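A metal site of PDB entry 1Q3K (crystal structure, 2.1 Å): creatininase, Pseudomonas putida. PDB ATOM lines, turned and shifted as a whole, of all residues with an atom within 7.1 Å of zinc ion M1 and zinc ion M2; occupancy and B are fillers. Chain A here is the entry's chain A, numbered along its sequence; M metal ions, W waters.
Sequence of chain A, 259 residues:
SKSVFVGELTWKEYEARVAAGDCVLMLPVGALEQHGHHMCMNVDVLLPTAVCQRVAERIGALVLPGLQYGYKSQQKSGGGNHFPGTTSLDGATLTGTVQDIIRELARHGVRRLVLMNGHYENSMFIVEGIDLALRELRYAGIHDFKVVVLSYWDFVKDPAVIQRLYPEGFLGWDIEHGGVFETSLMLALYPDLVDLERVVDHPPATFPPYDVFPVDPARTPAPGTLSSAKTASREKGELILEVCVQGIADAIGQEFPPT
The backbone carbonyl oxygen (O) of Gly 78 lies within hydrogen-bond range of a ring nitrogen (NE2) of His 177, at 3.0 Å. A ring nitrogen (NE2) of His 119 lies within hydrogen-bond range of the backbone carbonyl oxygen (O) of Tyr 71 (2.9 Å). A ring nitrogen (NE2) of His 177 is in hydrogen-bond range of the backbone carbonyl oxygen of Gln 34. The side-chain carboxylate (OE2) of Glu 33 is in hydrogen-bond range of the side-chain hydroxyl (OG) of Ser 73 (2.6 Å). The side-chain carboxylate (OE1) of Glu 182 is in hydrogen-bond range of the backbone NH (N) of Gly 178 (2.7 Å). ND1 of His 35 lies within hydrogen-bond range of O of Glu 33 (2.7 Å). A ring nitrogen (NE2) of His 119 lies close to the side-chain carboxylate of Glu 121 (3.4 Å).
Within 4 Å of zinc ion M2: Glu 33, Asp 44 and His 119.
Zinc ion M2 is bound by OD2 of Asp 44, at 1.9 Å. OE1 of Glu 33 binds zinc ion M2 (2.0 Å). A ring nitrogen (ND1) of His 119 binds zinc ion M2, at 2.4 Å. Water W3 is bound to zinc ion M2, 2.4 Å away. Zinc ion M2 is bound by water W2. Water W1 is bound to zinc ion M2 (2.7 Å). Zinc ion M2 has six donor atoms within binding distance.
Zinc ion M1 is bound by OE2 of Glu 182, water W2, OD1 of Asp 44 and NE2 of His 35. Zinc ion M1 has four donor atoms within binding distance. Slightly farther from zinc ion M1 lies OE1 of Glu 182 (2.8 Å).
Water W2 bridges ND1 of His 177 (2.5 Å) and OE1 of Glu 182 (3.5 Å).
Residues that only touch zinc ion M1: His 177 (3.9 Å). Four residues have an atom within 4 Å of zinc ion M1: His 35, Asp 44, His 177 and Glu 182.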
ATOM      1  N   GLY A  30     -15.238  28.635 -29.182  1.00  0.00           N
ATOM      2  CA  GLY A  30     -16.311  28.089 -28.350  1.00  0.00           C
ATOM      3  C   GLY A  30     -16.013  28.045 -26.844  1.00  0.00           C
ATOM      4  O   GLY A  30     -15.496  28.993 -26.296  1.00  0.00           O
ATOM      5  N   ALA A  31     -16.338  26.920 -26.211  1.00  0.00           N
ATOM      6  CA  ALA A  31     -16.185  26.726 -24.778  1.00  0.00           C
ATOM      7  C   ALA A  31     -16.441  25.276 -24.406  1.00  0.00           C
ATOM      8  O   ALA A  31     -16.903  24.493 -25.240  1.00  0.00           O
ATOM      9  CB  ALA A  31     -17.130  27.608 -24.047  1.00  0.00           C
ATOM     10  N   GLU A  33     -18.510  23.834 -21.660  1.00  0.00           N
ATOM     11  CA  GLU A  33     -19.518  24.245 -20.732  1.00  0.00           C
ATOM     12  C   GLU A  33     -20.738  23.288 -20.607  1.00  0.00           C
ATOM     13  O   GLU A  33     -21.229  22.721 -21.564  1.00  0.00           O
ATOM     14  CB  GLU A  33     -19.989  25.641 -21.194  1.00  0.00           C
ATOM     15  CG  GLU A  33     -21.089  26.316 -20.422  1.00  0.00           C
ATOM     16  CD  GLU A  33     -21.582  27.538 -21.138  1.00  0.00           C
ATOM     17  OE1 GLU A  33     -21.745  27.486 -22.382  1.00  0.00           O
ATOM     18  OE2 GLU A  33     -21.844  28.596 -20.501  1.00  0.00           O
ATOM     19  N   GLN A  34     -21.202  23.088 -19.385  1.00  0.00           N
ATOM     20  CA  GLN A  34     -22.358  22.261 -19.125  1.00  0.00           C
ATOM     21  C   GLN A  34     -23.522  22.749 -20.005  1.00  0.00           C
ATOM     22  O   GLN A  34     -23.699  23.955 -20.245  1.00  0.00           O
ATOM     23  CB  GLN A  34     -22.749  22.338 -17.656  1.00  0.00           C
ATOM     24  CG  GLN A  34     -23.211  23.680 -17.181  1.00  0.00           C
ATOM     25  CD  GLN A  34     -24.636  24.019 -17.552  1.00  0.00           C
ATOM     26  OE1 GLN A  34     -25.031  25.227 -17.553  1.00  0.00           O
ATOM     27  NE2 GLN A  34     -25.436  23.021 -17.843  1.00  0.00           N
ATOM     28  N   HIS A  35     -24.273  21.807 -20.537  1.00  0.00           N
ATOM     29  CA  HIS A  35     -25.405  22.104 -21.368  1.00  0.00           C
ATOM     30  C   HIS A  35     -26.565  21.204 -20.922  1.00  0.00           C
ATOM     31  O   HIS A  35     -27.120  20.455 -21.713  1.00  0.00           O
ATOM     32  CB  HIS A  35     -25.071  21.878 -22.852  1.00  0.00           C
ATOM     33  CG  HIS A  35     -24.480  23.098 -23.513  1.00  0.00           C
ATOM     34  ND1 HIS A  35     -23.178  23.495 -23.294  1.00  0.00           N
ATOM     35  CD2 HIS A  35     -25.027  24.016 -24.327  1.00  0.00           C
ATOM     36  CE1 HIS A  35     -22.934  24.582 -23.992  1.00  0.00           C
ATOM     37  NE2 HIS A  35     -24.044  24.923 -24.626  1.00  0.00           N
ATOM     38  N   MET A  39     -27.329  17.109 -23.185  1.00  0.00           N
ATOM     39  CA  MET A  39     -26.277  17.289 -24.214  1.00  0.00           C
ATOM     40  C   MET A  39     -24.872  17.281 -23.615  1.00  0.00           C
ATOM     41  O   MET A  39     -24.666  17.534 -22.438  1.00  0.00           O
ATOM     42  CB  MET A  39     -26.422  18.613 -24.953  1.00  0.00           C
ATOM     43  CG  MET A  39     -27.503  18.660 -25.962  1.00  0.00           C
ATOM     44  SD  MET A  39     -27.360  20.123 -26.989  1.00  0.00           S
ATOM     45  CE  MET A  39     -27.741  21.403 -25.831  1.00  0.00           C
ATOM     46  N   VAL A  43     -20.550  21.516 -27.084  1.00  0.00           N
ATOM     47  CA  VAL A  43     -21.519  22.084 -28.014  1.00  0.00           C
ATOM     48  C   VAL A  43     -21.028  23.387 -28.645  1.00  0.00           C
ATOM     49  O   VAL A  43     -20.991  23.519 -29.860  1.00  0.00           O
ATOM     50  CB  VAL A  43     -22.824  22.337 -27.281  1.00  0.00           C
ATOM     51  CG1 VAL A  43     -23.788  23.126 -28.121  1.00  0.00           C
ATOM     52  CG2 VAL A  43     -23.466  21.031 -26.849  1.00  0.00           C
ATOM     53  N   ASP A  44     -20.633  24.340 -27.790  1.00  0.00           N
ATOM     54  CA  ASP A  44     -20.180  25.678 -28.248  1.00  0.00           C
ATOM     55  C   ASP A  44     -18.981  25.610 -29.181  1.00  0.00           C
ATOM     56  O   ASP A  44     -18.724  26.548 -29.934  1.00  0.00           O
ATOM     57  CB  ASP A  44     -19.914  26.623 -27.078  1.00  0.00           C
ATOM     58  CG  ASP A  44     -21.181  27.021 -26.352  1.00  0.00           C
ATOM     59  OD1 ASP A  44     -22.207  26.497 -26.813  1.00  0.00           O
ATOM     60  OD2 ASP A  44     -21.245  27.803 -25.338  1.00  0.00           O
ATOM     61  N   VAL A  45     -18.270  24.503 -29.194  1.00  0.00           N
ATOM     62  CA  VAL A  45     -17.151  24.367 -30.112  1.00  0.00           C
ATOM     63  C   VAL A  45     -17.623  23.581 -31.366  1.00  0.00           C
ATOM     64  O   VAL A  45     -17.301  23.943 -32.531  1.00  0.00           O
ATOM     65  CB  VAL A  45     -15.992  23.610 -29.461  1.00  0.00           C
ATOM     66  CG1 VAL A  45     -14.898  23.457 -30.438  1.00  0.00           C
ATOM     67  CG2 VAL A  45     -15.462  24.352 -28.246  1.00  0.00           C
ATOM     68  N   LEU A  47     -20.720  23.221 -32.686  1.00  0.00           N
ATOM     69  CA  LEU A  47     -21.649  23.935 -33.512  1.00  0.00           C
ATOM     70  C   LEU A  47     -20.949  24.942 -34.425  1.00  0.00           C
ATOM     71  O   LEU A  47     -21.110  24.845 -35.634  1.00  0.00           O
ATOM     72  CB  LEU A  47     -22.731  24.648 -32.688  1.00  0.00           C
ATOM     73  CG  LEU A  47     -23.582  23.604 -31.957  1.00  0.00           C
ATOM     74  CD1 LEU A  47     -24.767  24.235 -31.253  1.00  0.00           C
ATOM     75  CD2 LEU A  47     -24.096  22.570 -32.966  1.00  0.00           C
ATOM     76  N   TYR A  71     -14.534  32.045 -22.286  1.00  0.00           N
ATOM     77  CA  TYR A  71     -14.680  32.838 -21.104  1.00  0.00           C
ATOM     78  C   TYR A  71     -15.676  32.189 -20.128  1.00  0.00           C
ATOM     79  O   TYR A  71     -16.538  31.373 -20.471  1.00  0.00           O
ATOM     80  CB  TYR A  71     -15.058  34.277 -21.410  1.00  0.00           C
ATOM     81  CG  TYR A  71     -15.040  35.130 -20.144  1.00  0.00           C
ATOM     82  CD1 TYR A  71     -13.864  35.346 -19.456  1.00  0.00           C
ATOM     83  CD2 TYR A  71     -16.206  35.639 -19.600  1.00  0.00           C
ATOM     84  CE1 TYR A  71     -13.831  36.053 -18.321  1.00  0.00           C
ATOM     85  CE2 TYR A  71     -16.148  36.383 -18.467  1.00  0.00           C
ATOM     86  CZ  TYR A  71     -14.960  36.541 -17.794  1.00  0.00           C
ATOM     87  OH  TYR A  71     -14.864  37.249 -16.630  1.00  0.00           O
ATOM     88  N   SER A  73     -18.529  31.193 -17.863  1.00  0.00           N
ATOM     89  CA  SER A  73     -19.957  31.136 -18.094  1.00  0.00           C
ATOM     90  C   SER A  73     -20.628  32.110 -17.116  1.00  0.00           C
ATOM     91  O   SER A  73     -20.320  32.155 -15.946  1.00  0.00           O
ATOM     92  CB  SER A  73     -20.454  29.644 -17.838  1.00  0.00           C
ATOM     93  OG  SER A  73     -21.831  29.563 -18.116  1.00  0.00           O
ATOM     94  N   SER A  77     -26.607  33.798 -19.190  1.00  0.00           N
ATOM     95  CA  SER A  77     -26.496  33.404 -20.574  1.00  0.00           C
ATOM     96  C   SER A  77     -25.990  32.004 -20.728  1.00  0.00           C
ATOM     97  O   SER A  77     -26.126  31.440 -21.805  1.00  0.00           O
ATOM     98  CB  SER A  77     -25.602  34.375 -21.344  1.00  0.00           C
ATOM     99  OG  SER A  77     -24.293  34.378 -20.769  1.00  0.00           O
ATOM    100  N   GLY A  78     -25.368  31.449 -19.716  1.00  0.00           N
ATOM    101  CA  GLY A  78     -24.815  30.098 -19.799  1.00  0.00           C
ATOM    102  C   GLY A  78     -24.988  29.267 -18.541  1.00  0.00           C
ATOM    103  O   GLY A  78     -24.527  28.160 -18.465  1.00  0.00           O
ATOM    104  N   GLY A 118     -19.142  30.690 -30.809  1.00  0.00           N
ATOM    105  CA  GLY A 118     -20.219  29.798 -30.452  1.00  0.00           C
ATOM    106  C   GLY A 118     -20.631  29.945 -28.980  1.00  0.00           C
ATOM    107  O   GLY A 118     -21.627  29.366 -28.523  1.00  0.00           O
ATOM    108  N   HIS A 119     -19.872  30.725 -28.226  1.00  0.00           N
ATOM    109  CA  HIS A 119     -20.109  30.925 -26.781  1.00  0.00           C
ATOM    110  C   HIS A 119     -20.349  32.433 -26.469  1.00  0.00           C
ATOM    111  O   HIS A 119     -19.447  33.270 -26.612  1.00  0.00           O
ATOM    112  CB  HIS A 119     -18.940  30.316 -26.000  1.00  0.00           C
ATOM    113  CG  HIS A 119     -18.996  30.484 -24.523  1.00  0.00           C
ATOM    114  ND1 HIS A 119     -20.006  29.985 -23.743  1.00  0.00           N
ATOM    115  CD2 HIS A 119     -18.115  31.060 -23.661  1.00  0.00           C
ATOM    116  CE1 HIS A 119     -19.779  30.267 -22.479  1.00  0.00           C
ATOM    117  NE2 HIS A 119     -18.652  30.952 -22.406  1.00  0.00           N
ATOM    118  N   TYR A 120     -21.593  32.768 -26.151  1.00  0.00           N
ATOM    119  CA  TYR A 120     -22.063  34.144 -25.891  1.00  0.00           C
ATOM    120  C   TYR A 120     -21.050  35.025 -25.118  1.00  0.00           C
ATOM    121  O   TYR A 120     -20.759  36.143 -25.479  1.00  0.00           O
ATOM    122  CB  TYR A 120     -23.342  34.047 -25.062  1.00  0.00           C
ATOM    123  CG  TYR A 120     -24.196  35.267 -25.037  1.00  0.00           C
ATOM    124  CD1 TYR A 120     -25.189  35.461 -26.010  1.00  0.00           C
ATOM    125  CD2 TYR A 120     -24.081  36.193 -24.017  1.00  0.00           C
ATOM    126  CE1 TYR A 120     -26.003  36.584 -25.979  1.00  0.00           C
ATOM    127  CE2 TYR A 120     -24.862  37.333 -23.980  1.00  0.00           C
ATOM    128  CZ  TYR A 120     -25.840  37.527 -24.965  1.00  0.00           C
ATOM    129  OH  TYR A 120     -26.641  38.678 -24.952  1.00  0.00           O
ATOM    130  N   GLU A 121     -20.541  34.481 -24.023  1.00  0.00           N
ATOM    131  CA  GLU A 121     -19.638  35.201 -23.171  1.00  0.00           C
ATOM    132  C   GLU A 121     -18.258  35.553 -23.764  1.00  0.00           C
ATOM    133  O   GLU A 121     -17.583  36.371 -23.209  1.00  0.00           O
ATOM    134  CB  GLU A 121     -19.456  34.421 -21.895  1.00  0.00           C
ATOM    135  CG  GLU A 121     -20.709  34.345 -21.083  1.00  0.00           C
ATOM    136  CD  GLU A 121     -21.550  33.101 -21.318  1.00  0.00           C
ATOM    137  OE1 GLU A 121     -21.625  32.647 -22.468  1.00  0.00           O
ATOM    138  OE2 GLU A 121     -22.151  32.619 -20.342  1.00  0.00           O
ATOM    139  N   TYR A 152     -22.764  32.902 -34.831  1.00  0.00           N
ATOM    140  CA  TYR A 152     -23.554  32.237 -35.863  1.00  0.00           C
ATOM    141  C   TYR A 152     -25.067  32.360 -35.640  1.00  0.00           C
ATOM    142  O   TYR A 152     -25.779  32.551 -36.586  1.00  0.00           O
ATOM    143  CB  TYR A 152     -23.119  30.758 -36.082  1.00  0.00           C
ATOM    144  CG  TYR A 152     -23.531  29.823 -34.966  1.00  0.00           C
ATOM    145  CD1 TYR A 152     -24.816  29.234 -34.937  1.00  0.00           C
ATOM    146  CD2 TYR A 152     -22.652  29.506 -33.938  1.00  0.00           C
ATOM    147  CE1 TYR A 152     -25.179  28.400 -33.893  1.00  0.00           C
ATOM    148  CE2 TYR A 152     -23.019  28.648 -32.913  1.00  0.00           C
ATOM    149  CZ  TYR A 152     -24.266  28.104 -32.887  1.00  0.00           C
ATOM    150  OH  TYR A 152     -24.620  27.290 -31.864  1.00  0.00           O
ATOM    151  N   TRP A 153     -25.560  32.325 -34.398  1.00  0.00           N
ATOM    152  CA  TRP A 153     -26.993  32.416 -34.188  1.00  0.00           C
ATOM    153  C   TRP A 153     -27.602  33.787 -34.596  1.00  0.00           C
ATOM    154  O   TRP A 153     -28.805  33.932 -34.832  1.00  0.00           O
ATOM    155  CB  TRP A 153     -27.364  32.097 -32.739  1.00  0.00           C
ATOM    156  CG  TRP A 153     -26.714  32.974 -31.746  1.00  0.00           C
ATOM    157  CD1 TRP A 153     -27.086  34.261 -31.409  1.00  0.00           C
ATOM    158  CD2 TRP A 153     -25.552  32.676 -30.940  1.00  0.00           C
ATOM    159  NE1 TRP A 153     -26.227  34.762 -30.458  1.00  0.00           N
ATOM    160  CE2 TRP A 153     -25.270  33.816 -30.168  1.00  0.00           C
ATOM    161  CE3 TRP A 153     -24.725  31.562 -30.815  1.00  0.00           C
ATOM    162  CZ2 TRP A 153     -24.211  33.855 -29.252  1.00  0.00           C
ATOM    163  CZ3 TRP A 153     -23.635  31.616 -29.909  1.00  0.00           C
ATOM    164  CH2 TRP A 153     -23.403  32.750 -29.150  1.00  0.00           C
ATOM    165  N   GLU A 176     -31.138  31.078 -24.528  1.00  0.00           N
ATOM    166  CA  GLU A 176     -30.972  29.987 -25.451  1.00  0.00           C
ATOM    167  C   GLU A 176     -29.773  29.118 -25.109  1.00  0.00           C
ATOM    168  O   GLU A 176     -28.960  28.791 -25.993  1.00  0.00           O
ATOM    169  CB  GLU A 176     -30.832  30.492 -26.875  1.00  0.00           C
ATOM    170  CG  GLU A 176     -32.149  30.620 -27.639  1.00  0.00           C
ATOM    171  CD  GLU A 176     -32.966  29.328 -27.670  1.00  0.00           C
ATOM    172  OE1 GLU A 176     -32.424  28.211 -27.810  1.00  0.00           O
ATOM    173  OE2 GLU A 176     -34.203  29.418 -27.568  1.00  0.00           O
ATOM    174  N   HIS A 177     -29.596  28.797 -23.828  1.00  0.00           N
ATOM    175  CA  HIS A 177     -28.464  27.986 -23.443  1.00  0.00           C
ATOM    176  C   HIS A 177     -28.941  26.581 -23.137  1.00  0.00           C
ATOM    177  O   HIS A 177     -29.541  26.329 -22.108  1.00  0.00           O
ATOM    178  CB  HIS A 177     -27.756  28.544 -22.208  1.00  0.00           C
ATOM    179  CG  HIS A 177     -26.710  27.619 -21.670  1.00  0.00           C
ATOM    180  ND1 HIS A 177     -25.541  27.344 -22.331  1.00  0.00           N
ATOM    181  CD2 HIS A 177     -26.662  26.919 -20.512  1.00  0.00           C
ATOM    182  CE1 HIS A 177     -24.807  26.521 -21.609  1.00  0.00           C
ATOM    183  NE2 HIS A 177     -25.468  26.238 -20.512  1.00  0.00           N
ATOM    184  N   GLY A 178     -28.595  25.667 -24.023  1.00  0.00           N
ATOM    185  CA  GLY A 178     -29.015  24.284 -23.900  1.00  0.00           C
ATOM    186  C   GLY A 178     -30.479  24.122 -24.295  1.00  0.00           C
ATOM    187  O   GLY A 178     -31.070  23.099 -24.066  1.00  0.00           O
ATOM    188  N   GLU A 182     -29.874  25.318 -29.816  1.00  0.00           N
ATOM    189  CA  GLU A 182     -28.687  24.461 -29.784  1.00  0.00           C
ATOM    190  C   GLU A 182     -29.007  22.946 -29.895  1.00  0.00           C
ATOM    191  O   GLU A 182     -28.385  22.225 -30.678  1.00  0.00           O
ATOM    192  CB  GLU A 182     -27.861  24.697 -28.517  1.00  0.00           C
ATOM    193  CG  GLU A 182     -27.216  26.071 -28.415  1.00  0.00           C
ATOM    194  CD  GLU A 182     -26.294  26.213 -27.200  1.00  0.00           C
ATOM    195  OE1 GLU A 182     -26.787  26.065 -26.047  1.00  0.00           O
ATOM    196  OE2 GLU A 182     -25.074  26.491 -27.419  1.00  0.00           O
HETATM  197 ZN    ZN M   1     -24.015  26.639 -25.881  1.00  0.00          ZN
HETATM  198 ZN    ZN M   2     -22.095  28.780 -23.885  1.00  0.00          ZN
HETATM  199  O   HOH W   1     -23.590  30.227 -25.555  1.00  0.00           O
HETATM  200  O   HOH W   2     -24.293  27.852 -24.440  1.00  0.00           O
HETATM  201  O   HOH W   3     -22.865  30.339 -22.208  1.00  0.00           O
